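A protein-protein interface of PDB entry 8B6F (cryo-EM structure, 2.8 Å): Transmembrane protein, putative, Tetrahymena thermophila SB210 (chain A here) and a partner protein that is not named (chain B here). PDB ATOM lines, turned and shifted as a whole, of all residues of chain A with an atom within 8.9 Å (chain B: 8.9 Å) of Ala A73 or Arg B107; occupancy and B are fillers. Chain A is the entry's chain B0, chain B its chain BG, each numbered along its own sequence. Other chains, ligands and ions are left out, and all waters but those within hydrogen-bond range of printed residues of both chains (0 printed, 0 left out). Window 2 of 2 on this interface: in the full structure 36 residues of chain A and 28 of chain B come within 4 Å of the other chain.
NH2 of Arg B107 is in hydrogen-bond range of OD1 of Asn B108 (3.2 Å). The backbone carbonyl oxygen (O) of Leu B104 sits at hydrogen-bond distance from the side-chain amide nitrogen (ND2) of Asn B108 (3.4 Å). The backbone carbonyl oxygen (O) of Lys A65 lies within hydrogen-bond range of the backbone NH (N) of Phe A70 (3.2 Å). O of Leu A66 lies within hydrogen-bond range of N of Lys A71 (3.2 Å).
The backbone carbonyl oxygen (O) of Ala A73 is in hydrogen-bond range of the guanidinium group (NE) of Arg B107 (3.3 Å).
Of the printed residues of chain B, Leu A66 touches Arg B100. Tyr A69 touches none of the printed residues of chain B. Of the printed residues of chain B, Phe A70 touches Arg B100 and Leu B104. Of chain B, only Leu B104 and Arg B107 come within 4 Å of Ala A73. Ile A74 touches just one residue of chain B: Leu B104. Printed residues of chain B within 4 Å of Trp A76: Arg B107 and Leu B111. Of the printed residues of chain A, Arg B100 touches Leu A66 and Phe A70. Of chain A, only Ala A73 (3.3 Å) and Trp A76 (3.8 Å) come within 4 Å of Arg B107. Printed residues of chain A within 4 Å of Leu B111: Trp A76 (3.6 Å). The nearest residue of chain B that does not touch Ala A73 is Asn B108 (6.5 Å). The nearest residue of chain A that does not touch Arg B107 is Ile A74 (4.1 Å).
Of the 16 printed residues of chain A, 5 touch a printed residue of chain B. Printed residues of chain A that touch a printed residue of chain B: Leu A66, Phe A70, Ala A73, Ile A74 and Trp A76. Of the 17 printed residues of chain B, 4 touch a printed residue of chain A. Printed residues of chain B that touch a printed residue of chain A: Arg B100, Leu B104, Arg B107 and Leu B111. Among the printed residues, no Asp or Glu carboxylate lies within 4 Å of a Lys or Arg side-chain nitrogen of the other chain.
Among the printed residues, pairs that only touch across the chains: Leu A66 with Arg B100 (3.3 Å), Phe A70 with Arg B100 (3.6 Å), Phe A70 with Leu B104 (3.2 Å), Ala A73 with Leu B104 (3.9 Å), Ile A74 with Leu B104 (3.8 Å), Trp A76 with Arg B107 (3.8 Å) and Trp A76 with Leu B111 (3.6 Å).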
ATOM      1  N   LYS A  65      -7.606  21.726 -28.082  1.00  0.00           N
ATOM      2  CA  LYS A  65      -8.633  20.693 -28.142  1.00  0.00           C
ATOM      3  C   LYS A  65      -8.037  19.320 -27.867  1.00  0.00           C
ATOM      4  O   LYS A  65      -8.609  18.527 -27.109  1.00  0.00           O
ATOM      5  CB  LYS A  65      -9.318  20.713 -29.509  1.00  0.00           C
ATOM      6  CG  LYS A  65     -10.153  21.956 -29.766  1.00  0.00           C
ATOM      7  CD  LYS A  65     -10.667  21.992 -31.195  1.00  0.00           C
ATOM      8  CE  LYS A  65     -11.465  23.258 -31.459  1.00  0.00           C
ATOM      9  NZ  LYS A  65     -11.952  23.330 -32.866  1.00  0.00           N
ATOM     10  N   LEU A  66      -6.889  19.020 -28.474  1.00  0.00           N
ATOM     11  CA  LEU A  66      -6.272  17.713 -28.277  1.00  0.00           C
ATOM     12  C   LEU A  66      -5.873  17.499 -26.823  1.00  0.00           C
ATOM     13  O   LEU A  66      -6.070  16.411 -26.271  1.00  0.00           O
ATOM     14  CB  LEU A  66      -5.059  17.563 -29.194  1.00  0.00           C
ATOM     15  CG  LEU A  66      -5.346  17.521 -30.698  1.00  0.00           C
ATOM     16  CD1 LEU A  66      -4.052  17.465 -31.481  1.00  0.00           C
ATOM     17  CD2 LEU A  66      -6.229  16.340 -31.062  1.00  0.00           C
ATOM     18  N   ARG A  67      -5.305  18.524 -26.183  1.00  0.00           N
ATOM     19  CA  ARG A  67      -4.821  18.358 -24.817  1.00  0.00           C
ATOM     20  C   ARG A  67      -5.958  18.307 -23.805  1.00  0.00           C
ATOM     21  O   ARG A  67      -5.832  17.639 -22.773  1.00  0.00           O
ATOM     22  CB  ARG A  67      -3.854  19.487 -24.460  1.00  0.00           C
ATOM     23  CG  ARG A  67      -2.431  19.258 -24.942  1.00  0.00           C
ATOM     24  CD  ARG A  67      -1.478  20.305 -24.384  1.00  0.00           C
ATOM     25  NE  ARG A  67      -1.748  21.636 -24.916  1.00  0.00           N
ATOM     26  CZ  ARG A  67      -1.194  22.135 -26.012  1.00  0.00           C
ATOM     27  NH1 ARG A  67      -0.325  21.441 -26.728  1.00  0.00           N
ATOM     28  NH2 ARG A  67      -1.522  23.363 -26.403  1.00  0.00           N
ATOM     29  N   HIS A  68      -7.067  18.997 -24.067  1.00  0.00           N
ATOM     30  CA  HIS A  68      -8.129  19.111 -23.077  1.00  0.00           C
ATOM     31  C   HIS A  68      -9.257  18.109 -23.263  1.00  0.00           C
ATOM     32  O   HIS A  68      -9.845  17.672 -22.269  1.00  0.00           O
ATOM     33  CB  HIS A  68      -8.721  20.524 -23.093  1.00  0.00           C
ATOM     34  CG  HIS A  68      -9.391  20.910 -21.812  1.00  0.00           C
ATOM     35  ND1 HIS A  68      -8.700  21.075 -20.632  1.00  0.00           N
ATOM     36  CD2 HIS A  68     -10.690  21.163 -21.524  1.00  0.00           C
ATOM     37  CE1 HIS A  68      -9.542  21.411 -19.672  1.00  0.00           C
ATOM     38  NE2 HIS A  68     -10.756  21.472 -20.187  1.00  0.00           N
ATOM     39  N   TYR A  69      -9.585  17.735 -24.498  1.00  0.00           N
ATOM     40  CA  TYR A  69     -10.741  16.884 -24.750  1.00  0.00           C
ATOM     41  C   TYR A  69     -10.369  15.538 -25.346  1.00  0.00           C
ATOM     42  O   TYR A  69     -10.841  14.502 -24.862  1.00  0.00           O
ATOM     43  CB  TYR A  69     -11.733  17.609 -25.676  1.00  0.00           C
ATOM     44  CG  TYR A  69     -12.486  18.723 -24.989  1.00  0.00           C
ATOM     45  CD1 TYR A  69     -13.686  18.474 -24.341  1.00  0.00           C
ATOM     46  CD2 TYR A  69     -11.991  20.020 -24.979  1.00  0.00           C
ATOM     47  CE1 TYR A  69     -14.377  19.485 -23.705  1.00  0.00           C
ATOM     48  CE2 TYR A  69     -12.674  21.037 -24.346  1.00  0.00           C
ATOM     49  CZ  TYR A  69     -13.867  20.763 -23.711  1.00  0.00           C
ATOM     50  OH  TYR A  69     -14.554  21.771 -23.079  1.00  0.00           O
ATOM     51  N   PHE A  70      -9.538  15.517 -26.387  1.00  0.00           N
ATOM     52  CA  PHE A  70      -9.248  14.262 -27.073  1.00  0.00           C
ATOM     53  C   PHE A  70      -8.598  13.252 -26.136  1.00  0.00           C
ATOM     54  O   PHE A  70      -9.021  12.092 -26.063  1.00  0.00           O
ATOM     55  CB  PHE A  70      -8.352  14.524 -28.282  1.00  0.00           C
ATOM     56  CG  PHE A  70      -7.696  13.292 -28.826  1.00  0.00           C
ATOM     57  CD1 PHE A  70      -8.378  12.443 -29.677  1.00  0.00           C
ATOM     58  CD2 PHE A  70      -6.387  12.989 -28.492  1.00  0.00           C
ATOM     59  CE1 PHE A  70      -7.769  11.310 -30.180  1.00  0.00           C
ATOM     60  CE2 PHE A  70      -5.773  11.860 -28.992  1.00  0.00           C
ATOM     61  CZ  PHE A  70      -6.465  11.019 -29.837  1.00  0.00           C
ATOM     62  N   LYS A  71      -7.569  13.674 -25.401  1.00  0.00           N
ATOM     63  CA  LYS A  71      -6.852  12.732 -24.545  1.00  0.00           C
ATOM     64  C   LYS A  71      -7.727  12.180 -23.432  1.00  0.00           C
ATOM     65  O   LYS A  71      -7.753  10.950 -23.250  1.00  0.00           O
ATOM     66  CB  LYS A  71      -5.591  13.399 -23.990  1.00  0.00           C
ATOM     67  CG  LYS A  71      -4.385  13.292 -24.913  1.00  0.00           C
ATOM     68  CD  LYS A  71      -3.879  11.859 -25.018  1.00  0.00           C
ATOM     69  CE  LYS A  71      -2.619  11.783 -25.860  1.00  0.00           C
ATOM     70  NZ  LYS A  71      -2.123  10.387 -25.994  1.00  0.00           N
ATOM     71  N   PRO A  72      -8.449  12.991 -22.659  1.00  0.00           N
ATOM     72  CA  PRO A  72      -9.390  12.401 -21.693  1.00  0.00           C
ATOM     73  C   PRO A  72     -10.435  11.521 -22.351  1.00  0.00           C
ATOM     74  O   PRO A  72     -10.819  10.490 -21.788  1.00  0.00           O
ATOM     75  CB  PRO A  72     -10.010  13.631 -21.017  1.00  0.00           C
ATOM     76  CG  PRO A  72      -8.991  14.697 -21.166  1.00  0.00           C
ATOM     77  CD  PRO A  72      -8.329  14.449 -22.490  1.00  0.00           C
ATOM     78  N   ALA A  73     -10.917  11.910 -23.532  1.00  0.00           N
ATOM     79  CA  ALA A  73     -11.933  11.114 -24.210  1.00  0.00           C
ATOM     80  C   ALA A  73     -11.401   9.735 -24.575  1.00  0.00           C
ATOM     81  O   ALA A  73     -12.107   8.730 -24.429  1.00  0.00           O
ATOM     82  CB  ALA A  73     -12.422  11.846 -25.459  1.00  0.00           C
ATOM     83  N   ILE A  74     -10.158   9.665 -25.050  1.00  0.00           N
ATOM     84  CA  ILE A  74      -9.599   8.399 -25.513  1.00  0.00           C
ATOM     85  C   ILE A  74      -8.993   7.571 -24.385  1.00  0.00           C
ATOM     86  O   ILE A  74      -8.813   6.357 -24.551  1.00  0.00           O
ATOM     87  CB  ILE A  74      -8.550   8.651 -26.616  1.00  0.00           C
ATOM     88  CG1 ILE A  74      -8.273   7.372 -27.409  1.00  0.00           C
ATOM     89  CG2 ILE A  74      -7.251   9.184 -26.028  1.00  0.00           C
ATOM     90  CD1 ILE A  74      -9.447   6.861 -28.213  1.00  0.00           C
ATOM     91  N   GLU A  75      -8.670   8.187 -23.251  1.00  0.00           N
ATOM     92  CA  GLU A  75      -8.211   7.471 -22.071  1.00  0.00           C
ATOM     93  C   GLU A  75      -9.313   7.296 -21.037  1.00  0.00           C
ATOM     94  O   GLU A  75      -9.032   6.889 -19.905  1.00  0.00           O
ATOM     95  CB  GLU A  75      -7.023   8.201 -21.441  1.00  0.00           C
ATOM     96  CG  GLU A  75      -5.869   8.476 -22.396  1.00  0.00           C
ATOM     97  CD  GLU A  75      -5.232   7.211 -22.940  1.00  0.00           C
ATOM     98  OE1 GLU A  75      -5.951   6.386 -23.541  1.00  0.00           O
ATOM     99  OE2 GLU A  75      -4.008   7.040 -22.765  1.00  0.00           O
ATOM    100  N   TRP A  76     -10.558   7.598 -21.399  1.00  0.00           N
ATOM    101  CA  TRP A  76     -11.661   7.512 -20.455  1.00  0.00           C
ATOM    102  C   TRP A  76     -11.826   6.094 -19.929  1.00  0.00           C
ATOM    103  O   TRP A  76     -11.688   5.115 -20.668  1.00  0.00           O
ATOM    104  CB  TRP A  76     -12.954   7.969 -21.123  1.00  0.00           C
ATOM    105  CG  TRP A  76     -14.159   7.849 -20.247  1.00  0.00           C
ATOM    106  CD1 TRP A  76     -14.525   8.686 -19.237  1.00  0.00           C
ATOM    107  CD2 TRP A  76     -15.165   6.831 -20.310  1.00  0.00           C
ATOM    108  NE1 TRP A  76     -15.694   8.253 -18.663  1.00  0.00           N
ATOM    109  CE2 TRP A  76     -16.108   7.115 -19.304  1.00  0.00           C
ATOM    110  CE3 TRP A  76     -15.358   5.706 -21.117  1.00  0.00           C
ATOM    111  CZ2 TRP A  76     -17.227   6.316 -19.084  1.00  0.00           C
ATOM    112  CZ3 TRP A  76     -16.469   4.913 -20.897  1.00  0.00           C
ATOM    113  CH2 TRP A  76     -17.390   5.222 -19.888  1.00  0.00           C
ATOM    114  N   GLN A  77     -12.127   5.993 -18.640  1.00  0.00           N
ATOM    115  CA  GLN A  77     -12.513   4.751 -17.995  1.00  0.00           C
ATOM    116  C   GLN A  77     -13.795   4.981 -17.211  1.00  0.00           C
ATOM    117  O   GLN A  77     -14.062   6.104 -16.773  1.00  0.00           O
ATOM    118  CB  GLN A  77     -11.418   4.240 -17.048  1.00  0.00           C
ATOM    119  CG  GLN A  77     -10.092   3.948 -17.727  1.00  0.00           C
ATOM    120  CD  GLN A  77     -10.162   2.754 -18.651  1.00  0.00           C
ATOM    121  OE1 GLN A  77     -11.216   2.148 -18.824  1.00  0.00           O
ATOM    122  NE2 GLN A  77      -9.031   2.405 -19.251  1.00  0.00           N
ATOM    123  N   PRO A  78     -14.603   3.939 -17.010  1.00  0.00           N
ATOM    124  CA  PRO A  78     -15.876   4.140 -16.299  1.00  0.00           C
ATOM    125  C   PRO A  78     -15.696   4.700 -14.902  1.00  0.00           C
ATOM    126  O   PRO A  78     -16.595   5.382 -14.396  1.00  0.00           O
ATOM    127  CB  PRO A  78     -16.494   2.735 -16.272  1.00  0.00           C
ATOM    128  CG  PRO A  78     -15.820   1.994 -17.368  1.00  0.00           C
ATOM    129  CD  PRO A  78     -14.432   2.541 -17.438  1.00  0.00           C
ATOM    130  N   TYR A  80     -13.107   6.725 -13.926  1.00  0.00           N
ATOM    131  CA  TYR A  80     -12.390   7.996 -13.885  1.00  0.00           C
ATOM    132  C   TYR A  80     -13.297   9.162 -13.522  1.00  0.00           C
ATOM    133  O   TYR A  80     -12.848  10.101 -12.857  1.00  0.00           O
ATOM    134  CB  TYR A  80     -11.710   8.282 -15.226  1.00  0.00           C
ATOM    135  CG  TYR A  80     -10.445   7.493 -15.467  1.00  0.00           C
ATOM    136  CD1 TYR A  80      -9.965   6.603 -14.517  1.00  0.00           C
ATOM    137  CD2 TYR A  80      -9.702   7.678 -16.624  1.00  0.00           C
ATOM    138  CE1 TYR A  80      -8.809   5.901 -14.721  1.00  0.00           C
ATOM    139  CE2 TYR A  80      -8.535   6.974 -16.839  1.00  0.00           C
ATOM    140  CZ  TYR A  80      -8.091   6.095 -15.871  1.00  0.00           C
ATOM    141  OH  TYR A  80      -6.939   5.374 -16.038  1.00  0.00           O
ATOM    142  N   THR A  88     -15.850  18.261 -16.449  1.00  0.00           N
ATOM    143  CA  THR A  88     -15.648  19.371 -17.367  1.00  0.00           C
ATOM    144  C   THR A  88     -16.896  19.585 -18.211  1.00  0.00           C
ATOM    145  O   THR A  88     -17.594  18.633 -18.569  1.00  0.00           O
ATOM    146  CB  THR A  88     -14.442  19.108 -18.270  1.00  0.00           C
ATOM    147  OG1 THR A  88     -14.677  17.937 -19.063  1.00  0.00           O
ATOM    148  CG2 THR A  88     -13.184  18.908 -17.438  1.00  0.00           C
ATOM    149  N   ARG B 100      -7.695  10.643 -35.637  1.00  0.00           N
ATOM    150  CA  ARG B 100      -8.128  10.757 -34.250  1.00  0.00           C
ATOM    151  C   ARG B 100      -9.631  10.546 -34.134  1.00  0.00           C
ATOM    152  O   ARG B 100     -10.104   9.856 -33.226  1.00  0.00           O
ATOM    153  CB  ARG B 100      -7.732  12.118 -33.684  1.00  0.00           C
ATOM    154  CG  ARG B 100      -6.233  12.338 -33.584  1.00  0.00           C
ATOM    155  CD  ARG B 100      -5.934  13.622 -32.836  1.00  0.00           C
ATOM    156  NE  ARG B 100      -4.504  13.844 -32.648  1.00  0.00           N
ATOM    157  CZ  ARG B 100      -3.738  14.564 -33.456  1.00  0.00           C
ATOM    158  NH1 ARG B 100      -4.226  15.146 -34.538  1.00  0.00           N
ATOM    159  NH2 ARG B 100      -2.451  14.716 -33.163  1.00  0.00           N
ATOM    160  N   HIS B 101     -10.396  11.138 -35.051  1.00  0.00           N
ATOM    161  CA  HIS B 101     -11.846  10.986 -35.028  1.00  0.00           C
ATOM    162  C   HIS B 101     -12.245   9.525 -35.181  1.00  0.00           C
ATOM    163  O   HIS B 101     -13.140   9.041 -34.481  1.00  0.00           O
ATOM    164  CB  HIS B 101     -12.462  11.836 -36.139  1.00  0.00           C
ATOM    165  CG  HIS B 101     -13.958  11.856 -36.133  1.00  0.00           C
ATOM    166  ND1 HIS B 101     -14.714  11.086 -36.988  1.00  0.00           N
ATOM    167  CD2 HIS B 101     -14.837  12.557 -35.380  1.00  0.00           C
ATOM    168  CE1 HIS B 101     -15.995  11.310 -36.762  1.00  0.00           C
ATOM    169  NE2 HIS B 101     -16.098  12.200 -35.793  1.00  0.00           N
ATOM    170  N   LEU B 102     -11.591   8.807 -36.095  1.00  0.00           N
ATOM    171  CA  LEU B 102     -11.901   7.397 -36.303  1.00  0.00           C
ATOM    172  C   LEU B 102     -11.475   6.540 -35.118  1.00  0.00           C
ATOM    173  O   LEU B 102     -12.136   5.541 -34.812  1.00  0.00           O
ATOM    174  CB  LEU B 102     -11.238   6.902 -37.587  1.00  0.00           C
ATOM    175  CG  LEU B 102     -11.760   7.544 -38.873  1.00  0.00           C
ATOM    176  CD1 LEU B 102     -10.922   7.115 -40.060  1.00  0.00           C
ATOM    177  CD2 LEU B 102     -13.222   7.193 -39.104  1.00  0.00           C
ATOM    178  N   ALA B 103     -10.383   6.902 -34.444  1.00  0.00           N
ATOM    179  CA  ALA B 103      -9.994   6.176 -33.240  1.00  0.00           C
ATOM    180  C   ALA B 103     -11.057   6.308 -32.158  1.00  0.00           C
ATOM    181  O   ALA B 103     -11.420   5.324 -31.505  1.00  0.00           O
ATOM    182  CB  ALA B 103      -8.644   6.684 -32.733  1.00  0.00           C
ATOM    183  N   LEU B 104     -11.559   7.526 -31.941  1.00  0.00           N
ATOM    184  CA  LEU B 104     -12.624   7.707 -30.960  1.00  0.00           C
ATOM    185  C   LEU B 104     -13.878   6.948 -31.371  1.00  0.00           C
ATOM    186  O   LEU B 104     -14.555   6.348 -30.528  1.00  0.00           O
ATOM    187  CB  LEU B 104     -12.930   9.193 -30.776  1.00  0.00           C
ATOM    188  CG  LEU B 104     -12.117   9.862 -29.666  1.00  0.00           C
ATOM    189  CD1 LEU B 104     -10.656   9.938 -30.052  1.00  0.00           C
ATOM    190  CD2 LEU B 104     -12.653  11.243 -29.340  1.00  0.00           C
ATOM    191  N   ARG B 105     -14.209   6.971 -32.664  1.00  0.00           N
ATOM    192  CA  ARG B 105     -15.372   6.232 -33.145  1.00  0.00           C
ATOM    193  C   ARG B 105     -15.209   4.735 -32.927  1.00  0.00           C
ATOM    194  O   ARG B 105     -16.164   4.048 -32.549  1.00  0.00           O
ATOM    195  CB  ARG B 105     -15.615   6.533 -34.623  1.00  0.00           C
ATOM    196  CG  ARG B 105     -16.400   7.813 -34.860  1.00  0.00           C
ATOM    197  CD  ARG B 105     -16.610   8.088 -36.341  1.00  0.00           C
ATOM    198  NE  ARG B 105     -17.275   6.985 -37.024  1.00  0.00           N
ATOM    199  CZ  ARG B 105     -17.620   6.997 -38.304  1.00  0.00           C
ATOM    200  NH1 ARG B 105     -17.384   8.046 -39.074  1.00  0.00           N
ATOM    201  NH2 ARG B 105     -18.221   5.930 -38.823  1.00  0.00           N
ATOM    202  N   GLU B 106     -14.004   4.206 -33.158  1.00  0.00           N
ATOM    203  CA  GLU B 106     -13.770   2.786 -32.921  1.00  0.00           C
ATOM    204  C   GLU B 106     -13.937   2.437 -31.449  1.00  0.00           C
ATOM    205  O   GLU B 106     -14.544   1.415 -31.113  1.00  0.00           O
ATOM    206  CB  GLU B 106     -12.375   2.391 -33.403  1.00  0.00           C
ATOM    207  CG  GLU B 106     -12.253   2.295 -34.914  1.00  0.00           C
ATOM    208  CD  GLU B 106     -10.882   1.831 -35.356  1.00  0.00           C
ATOM    209  OE1 GLU B 106      -9.977   1.757 -34.499  1.00  0.00           O
ATOM    210  OE2 GLU B 106     -10.709   1.533 -36.557  1.00  0.00           O
ATOM    211  N   ARG B 107     -13.408   3.272 -30.555  1.00  0.00           N
ATOM    212  CA  ARG B 107     -13.592   3.026 -29.130  1.00  0.00           C
ATOM    213  C   ARG B 107     -15.073   3.011 -28.775  1.00  0.00           C
ATOM    214  O   ARG B 107     -15.544   2.123 -28.055  1.00  0.00           O
ATOM    215  CB  ARG B 107     -12.851   4.084 -28.313  1.00  0.00           C
ATOM    216  CG  ARG B 107     -12.949   3.878 -26.809  1.00  0.00           C
ATOM    217  CD  ARG B 107     -12.389   5.062 -26.044  1.00  0.00           C
ATOM    218  NE  ARG B 107     -13.116   6.293 -26.338  1.00  0.00           N
ATOM    219  CZ  ARG B 107     -14.261   6.645 -25.771  1.00  0.00           C
ATOM    220  NH1 ARG B 107     -14.852   5.875 -24.873  1.00  0.00           N
ATOM    221  NH2 ARG B 107     -14.826   7.797 -26.113  1.00  0.00           N
ATOM    222  N   ASN B 108     -15.826   3.993 -29.274  1.00  0.00           N
ATOM    223  CA  ASN B 108     -17.252   4.058 -28.971  1.00  0.00           C
ATOM    224  C   ASN B 108     -17.990   2.858 -29.547  1.00  0.00           C
ATOM    225  O   ASN B 108     -18.903   2.319 -28.912  1.00  0.00           O
ATOM    226  CB  ASN B 108     -17.847   5.360 -29.507  1.00  0.00           C
ATOM    227  CG  ASN B 108     -17.560   6.543 -28.609  1.00  0.00           C
ATOM    228  OD1 ASN B 108     -17.462   6.404 -27.392  1.00  0.00           O
ATOM    229  ND2 ASN B 108     -17.428   7.719 -29.206  1.00  0.00           N
ATOM    230  N   ASP B 109     -17.614   2.426 -30.751  1.00  0.00           N
ATOM    231  CA  ASP B 109     -18.261   1.260 -31.341  1.00  0.00           C
ATOM    232  C   ASP B 109     -18.001   0.012 -30.508  1.00  0.00           C
ATOM    233  O   ASP B 109     -18.912  -0.791 -30.280  1.00  0.00           O
ATOM    234  CB  ASP B 109     -17.775   1.057 -32.776  1.00  0.00           C
ATOM    235  CG  ASP B 109     -18.171   2.199 -33.693  1.00  0.00           C
ATOM    236  OD1 ASP B 109     -18.843   3.138 -33.219  1.00  0.00           O
ATOM    237  OD2 ASP B 109     -17.810   2.158 -34.888  1.00  0.00           O
ATOM    238  N   MET B 110     -16.763  -0.173 -30.046  1.00  0.00           N
ATOM    239  CA  MET B 110     -16.461  -1.319 -29.197  1.00  0.00           C
ATOM    240  C   MET B 110     -17.276  -1.274 -27.912  1.00  0.00           C
ATOM    241  O   MET B 110     -17.841  -2.287 -27.486  1.00  0.00           O
ATOM    242  CB  MET B 110     -14.966  -1.352 -28.879  1.00  0.00           C
ATOM    243  CG  MET B 110     -14.094  -1.765 -30.050  1.00  0.00           C
ATOM    244  SD  MET B 110     -12.338  -1.492 -29.739  1.00  0.00           S
ATOM    245  CE  MET B 110     -12.111  -2.390 -28.209  1.00  0.00           C
ATOM    246  N   LEU B 111     -17.342  -0.104 -27.276  1.00  0.00           N
ATOM    247  CA  LEU B 111     -18.102   0.013 -26.036  1.00  0.00           C
ATOM    248  C   LEU B 111     -19.578  -0.277 -26.274  1.00  0.00           C
ATOM    249  O   LEU B 111     -20.207  -1.010 -25.501  1.00  0.00           O
ATOM    250  CB  LEU B 111     -17.911   1.405 -25.434  1.00  0.00           C
ATOM    251  CG  LEU B 111     -18.656   1.680 -24.124  1.00  0.00           C
ATOM    252  CD1 LEU B 111     -17.797   2.496 -23.182  1.00  0.00           C
ATOM    253  CD2 LEU B 111     -19.970   2.393 -24.378  1.00  0.00           C
ATOM    254  N   TYR B 112     -20.147   0.281 -27.346  1.00  0.00           N
ATOM    255  CA  TYR B 112     -21.558   0.052 -27.637  1.00  0.00           C
ATOM    256  C   TYR B 112     -21.833  -1.419 -27.914  1.00  0.00           C
ATOM    257  O   TYR B 112     -22.820  -1.977 -27.421  1.00  0.00           O
ATOM    258  CB  TYR B 112     -22.000   0.901 -28.832  1.00  0.00           C
ATOM    259  CG  TYR B 112     -22.000   2.397 -28.596  1.00  0.00           C
ATOM    260  CD1 TYR B 112     -21.669   2.934 -27.359  1.00  0.00           C
ATOM    261  CD2 TYR B 112     -22.348   3.273 -29.616  1.00  0.00           C
ATOM    262  CE1 TYR B 112     -21.677   4.299 -27.146  1.00  0.00           C
ATOM    263  CE2 TYR B 112     -22.359   4.640 -29.414  1.00  0.00           C
ATOM    264  CZ  TYR B 112     -22.023   5.147 -28.177  1.00  0.00           C
ATOM    265  OH  TYR B 112     -22.033   6.507 -27.971  1.00  0.00           O
ATOM    266  N   ASN B 113     -20.971  -2.068 -28.697  1.00  0.00           N
ATOM    267  CA  ASN B 113     -21.167  -3.485 -28.983  1.00  0.00           C
ATOM    268  C   ASN B 113     -21.118  -4.315 -27.708  1.00  0.00           C
ATOM    269  O   ASN B 113     -21.956  -5.200 -27.504  1.00  0.00           O
ATOM    270  CB  ASN B 113     -20.112  -3.972 -29.977  1.00  0.00           C
ATOM    271  CG  ASN B 113     -20.302  -3.386 -31.361  1.00  0.00           C
ATOM    272  OD1 ASN B 113     -21.423  -3.099 -31.778  1.00  0.00           O
ATOM    273  ND2 ASN B 113     -19.202  -3.207 -32.084  1.00  0.00           N
ATOM    274  N   GLU B 114     -20.141  -4.049 -26.839  1.00  0.00           N
ATOM    275  CA  GLU B 114     -20.047  -4.811 -25.600  1.00  0.00           C
ATOM    276  C   GLU B 114     -21.275  -4.598 -24.725  1.00  0.00           C
ATOM    277  O   GLU B 114     -21.788  -5.546 -24.120  1.00  0.00           O
ATOM    278  CB  GLU B 114     -18.781  -4.420 -24.838  1.00  0.00           C
ATOM    279  CG  GLU B 114     -18.515  -5.279 -23.614  1.00  0.00           C
ATOM    280  CD  GLU B 114     -18.280  -6.734 -23.969  1.00  0.00           C
ATOM    281  OE1 GLU B 114     -17.666  -6.998 -25.022  1.00  0.00           O
ATOM    282  OE2 GLU B 114     -18.719  -7.614 -23.199  1.00  0.00           O
ATOM    283  N   LEU B 115     -21.763  -3.358 -24.643  1.00  0.00           N
ATOM    284  CA  LEU B 115     -22.875  -3.063 -23.747  1.00  0.00           C
ATOM    285  C   LEU B 115     -24.190  -3.623 -24.277  1.00  0.00           C
ATOM    286  O   LEU B 115     -25.035  -4.075 -23.496  1.00  0.00           O
ATOM    287  CB  LEU B 115     -22.989  -1.554 -23.529  1.00  0.00           C
ATOM    288  CG  LEU B 115     -21.878  -0.872 -22.725  1.00  0.00           C
ATOM    289  CD1 LEU B 115     -22.162   0.613 -22.583  1.00  0.00           C
ATOM    290  CD2 LEU B 115     -21.706  -1.506 -21.355  1.00  0.00           C
ATOM    291  N   GLN B 128     -27.665   0.564 -33.256  1.00  0.00           N
ATOM    292  CA  GLN B 128     -26.587   1.376 -33.810  1.00  0.00           C
ATOM    293  C   GLN B 128     -26.970   1.979 -35.157  1.00  0.00           C
ATOM    294  O   GLN B 128     -26.623   3.130 -35.444  1.00  0.00           O
ATOM    295  CB  GLN B 128     -25.316   0.537 -33.932  1.00  0.00           C
ATOM    296  CG  GLN B 128     -24.705   0.170 -32.586  1.00  0.00           C
ATOM    297  CD  GLN B 128     -23.421  -0.622 -32.725  1.00  0.00           C
ATOM    298  OE1 GLN B 128     -22.941  -0.860 -33.831  1.00  0.00           O
ATOM    299  NE2 GLN B 128     -22.859  -1.035 -31.595  1.00  0.00           N
